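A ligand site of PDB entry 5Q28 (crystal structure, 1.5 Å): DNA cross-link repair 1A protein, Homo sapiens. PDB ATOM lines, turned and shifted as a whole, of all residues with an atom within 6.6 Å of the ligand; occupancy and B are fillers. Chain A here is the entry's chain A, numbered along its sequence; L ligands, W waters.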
ATOM      1  N   LYS A 304      -7.449 -23.925  -9.697  1.00  0.00           N
ATOM      2  CA  LYS A 304      -6.506 -24.766  -8.947  1.00  0.00           C
ATOM      3  C   LYS A 304      -6.225 -26.123  -9.620  1.00  0.00           C
ATOM      4  O   LYS A 304      -5.051 -26.556  -9.736  1.00  0.00           O
ATOM      5  CB  LYS A 304      -6.997 -24.981  -7.509  1.00  0.00           C
ATOM      6  CG  LYS A 304      -6.199 -25.916  -6.627  1.00  0.00           C
ATOM      7  CD  LYS A 304      -6.810 -25.902  -5.208  1.00  0.00           C
ATOM      8  CE  LYS A 304      -6.070 -26.768  -4.198  1.00  0.00           C
ATOM      9  NZ  LYS A 304      -6.245 -28.181  -4.547  1.00  0.00           N
ATOM     10  N   VAL A 307      -4.039 -25.674 -12.892  1.00  0.00           N
ATOM     11  CA  VAL A 307      -2.645 -25.358 -12.588  1.00  0.00           C
ATOM     12  C   VAL A 307      -1.902 -26.542 -11.959  1.00  0.00           C
ATOM     13  O   VAL A 307      -0.748 -26.758 -12.302  1.00  0.00           O
ATOM     14  CB  VAL A 307      -2.544 -24.067 -11.762  1.00  0.00           C
ATOM     15  CG1 VAL A 307      -1.082 -23.748 -11.363  1.00  0.00           C
ATOM     16  CG2 VAL A 307      -3.133 -22.856 -12.519  1.00  0.00           C
ATOM     17  N   GLN A 308      -2.543 -27.323 -11.063  1.00  0.00           N
ATOM     18  CA  GLN A 308      -1.882 -28.502 -10.453  1.00  0.00           C
ATOM     19  C   GLN A 308      -1.692 -29.614 -11.484  1.00  0.00           C
ATOM     20  O   GLN A 308      -0.764 -30.434 -11.357  1.00  0.00           O
ATOM     21  CB  GLN A 308      -2.649 -29.020  -9.233  1.00  0.00           C
ATOM     22  CG  GLN A 308      -2.633 -28.082  -8.028  1.00  0.00           C
ATOM     23  CD  GLN A 308      -3.429 -28.589  -6.835  1.00  0.00           C
ATOM     24  OE1 GLN A 308      -4.586 -29.028  -6.965  1.00  0.00           O
ATOM     25  NE2 GLN A 308      -2.819 -28.515  -5.656  1.00  0.00           N
ATOM     26  N   TRP A 309      -2.552 -29.648 -12.524  1.00  0.00           N
ATOM     27  CA  TRP A 309      -2.360 -30.584 -13.637  1.00  0.00           C
ATOM     28  C   TRP A 309      -1.183 -30.157 -14.544  1.00  0.00           C
ATOM     29  O   TRP A 309      -0.278 -30.972 -14.864  1.00  0.00           O
ATOM     30  CB  TRP A 309      -3.675 -30.762 -14.465  1.00  0.00           C
ATOM     31  CG  TRP A 309      -3.451 -31.564 -15.734  1.00  0.00           C
ATOM     32  CD1 TRP A 309      -3.384 -32.926 -15.830  1.00  0.00           C
ATOM     33  CD2 TRP A 309      -3.222 -31.067 -17.053  1.00  0.00           C
ATOM     34  NE1 TRP A 309      -3.132 -33.302 -17.110  1.00  0.00           N
ATOM     35  CE2 TRP A 309      -3.022 -32.190 -17.894  1.00  0.00           C
ATOM     36  CE3 TRP A 309      -3.183 -29.791 -17.613  1.00  0.00           C
ATOM     37  CZ2 TRP A 309      -2.772 -32.070 -19.265  1.00  0.00           C
ATOM     38  CZ3 TRP A 309      -2.929 -29.667 -18.996  1.00  0.00           C
ATOM     39  CH2 TRP A 309      -2.739 -30.802 -19.798  1.00  0.00           C
ATOM     40  N   LEU A 310      -1.206 -28.903 -14.959  1.00  0.00           N
ATOM     41  CA  LEU A 310      -0.178 -28.332 -15.874  1.00  0.00           C
ATOM     42  C   LEU A 310       1.265 -28.296 -15.286  1.00  0.00           C
ATOM     43  O   LEU A 310       2.227 -28.573 -15.995  1.00  0.00           O
ATOM     44  CB  LEU A 310      -0.607 -26.929 -16.331  1.00  0.00           C
ATOM     45  CG  LEU A 310       0.138 -26.292 -17.489  1.00  0.00           C
ATOM     46  CD1 LEU A 310      -0.183 -26.977 -18.823  1.00  0.00           C
ATOM     47  CD2 LEU A 310      -0.199 -24.810 -17.547  1.00  0.00           C
ATOM     48  N   LYS A 311       1.373 -28.013 -13.988  1.00  0.00           N
ATOM     49  CA  LYS A 311       2.647 -27.893 -13.257  1.00  0.00           C
ATOM     50  C   LYS A 311       3.709 -27.001 -13.941  1.00  0.00           C
ATOM     51  O   LYS A 311       4.856 -27.442 -14.181  1.00  0.00           O
ATOM     52  CB  LYS A 311       3.221 -29.286 -12.965  1.00  0.00           C
ATOM     53  CG  LYS A 311       2.274 -30.184 -12.170  1.00  0.00           C
ATOM     54  CD  LYS A 311       2.809 -31.603 -12.102  1.00  0.00           C
ATOM     55  CE  LYS A 311       2.163 -32.430 -11.008  1.00  0.00           C
ATOM     56  NZ  LYS A 311       0.782 -32.858 -11.390  1.00  0.00           N
ATOM     57  N   PRO A 312       3.384 -25.706 -14.169  1.00  0.00           N
ATOM     58  CA  PRO A 312       4.332 -24.770 -14.762  1.00  0.00           C
ATOM     59  C   PRO A 312       5.475 -24.423 -13.819  1.00  0.00           C
ATOM     60  O   PRO A 312       5.335 -24.606 -12.608  1.00  0.00           O
ATOM     61  CB  PRO A 312       3.455 -23.530 -15.019  1.00  0.00           C
ATOM     62  CG  PRO A 312       2.467 -23.568 -13.904  1.00  0.00           C
ATOM     63  CD  PRO A 312       2.154 -25.012 -13.712  1.00  0.00           C
ATOM     64  N   GLN A 313       6.595 -23.943 -14.365  1.00  0.00           N
ATOM     65  CA  GLN A 313       7.734 -23.511 -13.549  1.00  0.00           C
ATOM     66  C   GLN A 313       7.565 -22.087 -13.010  1.00  0.00           C
ATOM     67  O   GLN A 313       8.053 -21.793 -11.915  1.00  0.00           O
ATOM     68  CB  GLN A 313       9.067 -23.630 -14.296  1.00  0.00           C
ATOM     69  CG  GLN A 313       9.469 -25.069 -14.666  1.00  0.00           C
ATOM     70  CD  GLN A 313      10.771 -25.145 -15.438  1.00  0.00           C
ATOM     71  OE1 GLN A 313      11.365 -24.124 -15.805  1.00  0.00           O
ATOM     72  NE2 GLN A 313      11.236 -26.357 -15.682  1.00  0.00           N
ATOM     73  N   LYS A 314       6.883 -21.226 -13.770  1.00  0.00           N
ATOM     74  CA  LYS A 314       6.600 -19.844 -13.388  1.00  0.00           C
ATOM     75  C   LYS A 314       5.124 -19.504 -13.729  1.00  0.00           C
ATOM     76  O   LYS A 314       4.603 -19.922 -14.764  1.00  0.00           O
ATOM     77  CB  LYS A 314       7.547 -18.888 -14.135  1.00  0.00           C
ATOM     78  CG  LYS A 314       7.496 -17.453 -13.631  1.00  0.00           C
ATOM     79  CD  LYS A 314       8.470 -16.527 -14.358  1.00  0.00           C
ATOM     80  N   ILE A 315       4.461 -18.769 -12.831  1.00  0.00           N
ATOM     81  CA  ILE A 315       3.069 -18.308 -13.052  1.00  0.00           C
ATOM     82  C   ILE A 315       3.091 -16.762 -12.990  1.00  0.00           C
ATOM     83  O   ILE A 315       3.632 -16.158 -12.044  1.00  0.00           O
ATOM     84  CB  ILE A 315       2.085 -18.870 -11.985  1.00  0.00           C
ATOM     85  CG1 ILE A 315       2.061 -20.401 -12.027  1.00  0.00           C
ATOM     86  CG2 ILE A 315       0.682 -18.292 -12.203  1.00  0.00           C
ATOM     87  CD1 ILE A 315       1.375 -21.059 -10.853  1.00  0.00           C
ATOM     88  N   ILE A 316       2.521 -16.130 -14.014  1.00  0.00           N
ATOM     89  CA  ILE A 316       2.435 -14.688 -14.150  1.00  0.00           C
ATOM     90  C   ILE A 316       0.935 -14.332 -14.218  1.00  0.00           C
ATOM     91  O   ILE A 316       0.282 -14.560 -15.243  1.00  0.00           O
ATOM     92  CB  ILE A 316       3.168 -14.205 -15.413  1.00  0.00           C
ATOM     93  CG1 ILE A 316       4.676 -14.503 -15.302  1.00  0.00           C
ATOM     94  CG2 ILE A 316       2.996 -12.709 -15.622  1.00  0.00           C
ATOM     95  CD1 ILE A 316       5.228 -15.265 -16.466  1.00  0.00           C
ATOM     96  N   PRO A 317       0.376 -13.763 -13.139  1.00  0.00           N
ATOM     97  CA  PRO A 317      -1.034 -13.369 -13.187  1.00  0.00           C
ATOM     98  C   PRO A 317      -1.289 -12.248 -14.145  1.00  0.00           C
ATOM     99  O   PRO A 317      -0.439 -11.339 -14.284  1.00  0.00           O
ATOM    100  CB  PRO A 317      -1.327 -12.853 -11.774  1.00  0.00           C
ATOM    101  CG  PRO A 317      -0.203 -13.292 -10.944  1.00  0.00           C
ATOM    102  CD  PRO A 317       0.981 -13.502 -11.819  1.00  0.00           C
ATOM    103  N   GLU A 331      -0.063 -15.070  -4.858  1.00  0.00           N
ATOM    104  CA  GLU A 331       1.232 -15.755  -4.701  1.00  0.00           C
ATOM    105  C   GLU A 331       1.185 -16.817  -3.611  1.00  0.00           C
ATOM    106  O   GLU A 331       1.719 -17.914  -3.779  1.00  0.00           O
ATOM    107  CB  GLU A 331       2.347 -14.769  -4.389  1.00  0.00           C
ATOM    108  CG  GLU A 331       2.793 -13.968  -5.603  1.00  0.00           C
ATOM    109  CD  GLU A 331       3.743 -12.837  -5.265  1.00  0.00           C
ATOM    110  OE1 GLU A 331       4.217 -12.153  -6.203  1.00  0.00           O
ATOM    111  OE2 GLU A 331       4.006 -12.614  -4.052  1.00  0.00           O
ATOM    112  N   PHE A 334      -0.736 -19.858  -4.986  1.00  0.00           N
ATOM    113  CA  PHE A 334       0.126 -20.615  -5.909  1.00  0.00           C
ATOM    114  C   PHE A 334       1.108 -21.541  -5.168  1.00  0.00           C
ATOM    115  O   PHE A 334       1.310 -22.703  -5.548  1.00  0.00           O
ATOM    116  CB  PHE A 334       0.901 -19.703  -6.852  1.00  0.00           C
ATOM    117  CG  PHE A 334       0.051 -18.740  -7.676  1.00  0.00           C
ATOM    118  CD1 PHE A 334      -1.271 -19.026  -8.090  1.00  0.00           C
ATOM    119  CD2 PHE A 334       0.611 -17.542  -8.089  1.00  0.00           C
ATOM    120  CE1 PHE A 334      -1.986 -18.107  -8.856  1.00  0.00           C
ATOM    121  CE2 PHE A 334      -0.110 -16.620  -8.863  1.00  0.00           C
ATOM    122  CZ  PHE A 334      -1.419 -16.910  -9.236  1.00  0.00           C
ATOM    123  N   ARG A 335       1.719 -21.009  -4.120  1.00  0.00           N
ATOM    124  CA  ARG A 335       2.626 -21.782  -3.245  1.00  0.00           C
ATOM    125  C   ARG A 335       1.900 -22.931  -2.554  1.00  0.00           C
ATOM    126  O   ARG A 335       2.436 -24.042  -2.489  1.00  0.00           O
ATOM    127  CB  ARG A 335       3.337 -20.866  -2.234  1.00  0.00           C
ATOM    128  CG  ARG A 335       4.224 -21.563  -1.202  1.00  0.00           C
ATOM    129  CD  ARG A 335       5.538 -22.042  -1.754  1.00  0.00           C
ATOM    130  NE  ARG A 335       6.558 -20.979  -1.740  1.00  0.00           N
ATOM    131  CZ  ARG A 335       7.809 -21.103  -2.197  1.00  0.00           C
ATOM    132  NH1 ARG A 335       8.630 -20.070  -2.129  1.00  0.00           N
ATOM    133  NH2 ARG A 335       8.244 -22.262  -2.715  1.00  0.00           N
ATOM    134  N   TRP A 337      -0.756 -24.474  -3.673  1.00  0.00           N
ATOM    135  CA  TRP A 337      -1.065 -25.471  -4.712  1.00  0.00           C
ATOM    136  C   TRP A 337       0.155 -26.344  -5.045  1.00  0.00           C
ATOM    137  O   TRP A 337       0.051 -27.554  -5.260  1.00  0.00           O
ATOM    138  CB  TRP A 337      -1.563 -24.820  -6.002  1.00  0.00           C
ATOM    139  CG  TRP A 337      -2.810 -23.947  -5.851  1.00  0.00           C
ATOM    140  CD1 TRP A 337      -3.656 -23.853  -4.788  1.00  0.00           C
ATOM    141  CD2 TRP A 337      -3.338 -23.080  -6.859  1.00  0.00           C
ATOM    142  NE1 TRP A 337      -4.661 -22.941  -5.043  1.00  0.00           N
ATOM    143  CE2 TRP A 337      -4.502 -22.470  -6.327  1.00  0.00           C
ATOM    144  CE3 TRP A 337      -2.924 -22.740  -8.173  1.00  0.00           C
ATOM    145  CZ2 TRP A 337      -5.257 -21.527  -7.058  1.00  0.00           C
ATOM    146  CZ3 TRP A 337      -3.708 -21.828  -8.897  1.00  0.00           C
ATOM    147  CH2 TRP A 337      -4.846 -21.234  -8.325  1.00  0.00           C
ATOM    148  N   LYS A 338       1.318 -25.694  -5.100  1.00  0.00           N
ATOM    149  CA  LYS A 338       2.576 -26.372  -5.394  1.00  0.00           C
ATOM    150  C   LYS A 338       2.937 -27.390  -4.299  1.00  0.00           C
ATOM    151  O   LYS A 338       3.296 -28.528  -4.609  1.00  0.00           O
ATOM    152  CB  LYS A 338       3.696 -25.339  -5.569  1.00  0.00           C
ATOM    153  CG  LYS A 338       5.055 -25.858  -6.015  1.00  0.00           C
ATOM    154  CD  LYS A 338       6.112 -24.729  -5.986  1.00  0.00           C
ATOM    155  CE  LYS A 338       7.557 -25.220  -5.974  1.00  0.00           C
ATOM    156  NZ  LYS A 338       8.204 -25.273  -7.320  1.00  0.00           N
ATOM    157  N   LEU A 339       2.821 -26.967  -3.038  1.00  0.00           N
ATOM    158  CA  LEU A 339       3.176 -27.837  -1.907  1.00  0.00           C
ATOM    159  C   LEU A 339       2.193 -29.020  -1.766  1.00  0.00           C
ATOM    160  O   LEU A 339       2.614 -30.151  -1.485  1.00  0.00           O
ATOM    161  CB  LEU A 339       3.234 -27.027  -0.616  1.00  0.00           C
ATOM    162  CG  LEU A 339       4.331 -25.961  -0.474  1.00  0.00           C
ATOM    163  CD1 LEU A 339       4.047 -25.043   0.716  1.00  0.00           C
ATOM    164  CD2 LEU A 339       5.694 -26.590  -0.313  1.00  0.00           C
ATOM    165  N   ALA A 341       0.637 -30.456  -4.170  1.00  0.00           N
ATOM    166  CA  ALA A 341       0.977 -31.386  -5.251  1.00  0.00           C
ATOM    167  C   ALA A 341       2.317 -32.151  -5.054  1.00  0.00           C
ATOM    168  O   ALA A 341       2.622 -33.051  -5.837  1.00  0.00           O
ATOM    169  CB  ALA A 341       0.989 -30.654  -6.575  1.00  0.00           C
ATOM    170  N   GLY A 342       3.107 -31.807  -4.035  1.00  0.00           N
ATOM    171  CA  GLY A 342       4.351 -32.511  -3.714  1.00  0.00           C
ATOM    172  C   GLY A 342       5.668 -31.854  -4.116  1.00  0.00           C
ATOM    173  O   GLY A 342       6.722 -32.477  -3.979  1.00  0.00           O
ATOM    174  N   TYR A 343       5.633 -30.610  -4.591  1.00  0.00           N
ATOM    175  CA  TYR A 343       6.856 -29.893  -5.021  1.00  0.00           C
ATOM    176  C   TYR A 343       7.296 -28.819  -4.024  1.00  0.00           C
ATOM    177  O   TYR A 343       6.585 -28.523  -3.068  1.00  0.00           O
ATOM    178  CB  TYR A 343       6.662 -29.223  -6.387  1.00  0.00           C
ATOM    179  CG  TYR A 343       6.400 -30.184  -7.518  1.00  0.00           C
ATOM    180  CD1 TYR A 343       5.155 -30.779  -7.665  1.00  0.00           C
ATOM    181  CD2 TYR A 343       7.382 -30.492  -8.453  1.00  0.00           C
ATOM    182  CE1 TYR A 343       4.890 -31.669  -8.690  1.00  0.00           C
ATOM    183  CE2 TYR A 343       7.129 -31.378  -9.496  1.00  0.00           C
ATOM    184  CZ  TYR A 343       5.876 -31.966  -9.597  1.00  0.00           C
ATOM    185  OH  TYR A 343       5.574 -32.838 -10.603  1.00  0.00           O
ATOM    186  OXT TYR A 343       8.367 -28.208  -4.160  1.00  0.00           O
HETATM  187  N1  LIG L   1       5.182 -19.138  -8.482  1.00  0.00           N
HETATM  188  C1  LIG L   1       5.200 -20.968 -10.002  1.00  0.00           C
HETATM  189  C2  LIG L   1       4.878 -22.242 -10.377  1.00  0.00           C
HETATM  190  C3  LIG L   1       4.103 -23.064  -9.574  1.00  0.00           C
HETATM  191  C4  LIG L   1       3.681 -22.571  -8.338  1.00  0.00           C
HETATM  192  C5  LIG L   1       4.021 -21.288  -7.934  1.00  0.00           C
HETATM  193  C6  LIG L   1       1.824 -25.345  -9.171  1.00  0.00           C
HETATM  194  C7  LIG L   1       2.988 -27.838  -9.461  1.00  0.00           C
HETATM  195  C8  LIG L   1       4.526 -16.887  -8.969  1.00  0.00           C
HETATM  196  C9  LIG L   1       5.305 -18.093  -9.352  1.00  0.00           C
HETATM  197  O1  LIG L   1       5.986 -18.111 -10.403  1.00  0.00           O
HETATM  198  C10 LIG L   1       4.801 -20.477  -8.769  1.00  0.00           C
HETATM  199  N2  LIG L   1       3.825 -24.325 -10.123  1.00  0.00           N
HETATM  200  C11 LIG L   1       3.106 -25.451  -9.691  1.00  0.00           C
HETATM  201  C12 LIG L   1       1.135 -26.479  -8.787  1.00  0.00           C
HETATM  202  C13 LIG L   1       1.712 -27.726  -8.929  1.00  0.00           C
HETATM  203  C14 LIG L   1       3.674 -26.706  -9.869  1.00  0.00           C
HETATM  204  O   HOH W   1       4.188 -17.974  -5.490  1.00  0.00           O
HETATM  205  O   HOH W   2       4.213 -14.021 -10.564  1.00  0.00           O
HETATM  206  O   HOH W   3       5.357 -20.586  -5.365  1.00  0.00           O
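The backbone carbonyl oxygen (O) of Pro 312 sits at hydrogen-bond distance from a nitrogen (N2) of the ligand (2.9 Å). The backbone NH (N) of Ile 315 sits at hydrogen-bond distance from an oxygen (O1) of the ligand, 2.9 Å away.
Water W1 lies within hydrogen-bond range of the backbone carbonyl oxygen (O) of Glu 331 (3.0 Å) and a nitrogen (N1) of the ligand (3.4 Å).
Residues that only touch the ligand: Lys 314 (3.5 Å), Gln 313 (3.5 Å), Lys 311 (3.7 Å), Phe 334 (3.7 Å), Lys 338 (3.7 Å), Ala 341 (3.8 Å), Trp 337 (3.8 Å), Val 307 (3.97 Å) and Gln 308 (3.98 Å). Hydrophobic or aromatic side chains within 4 Å of the ligand: Val 307, Ile 315, Phe 334 and Ala 341. Of the 21 residues printed, 11 come within 4 Å of the ligand. The nearest printed residue that does not touch the ligand is Tyr 343 (4.1 Å).
The side-chain amino group (NZ) of Lys 311 is in hydrogen-bond range of the backbone carbonyl oxygen (O) of Gln 308 (2.9 Å). The backbone NH (N) of Tyr 343 lies within hydrogen-bond range of the backbone carbonyl oxygen (O) of Lys 338, 3.1 Å away. The backbone carbonyl oxygen (O) of Trp 337 is in hydrogen-bond range of the side-chain amide nitrogen (NE2) of Gln 308 (3.1 Å). The side-chain amino group of Lys 304 is in hydrogen-bond range of the side-chain amide oxygen of Gln 308 (3.1 Å).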
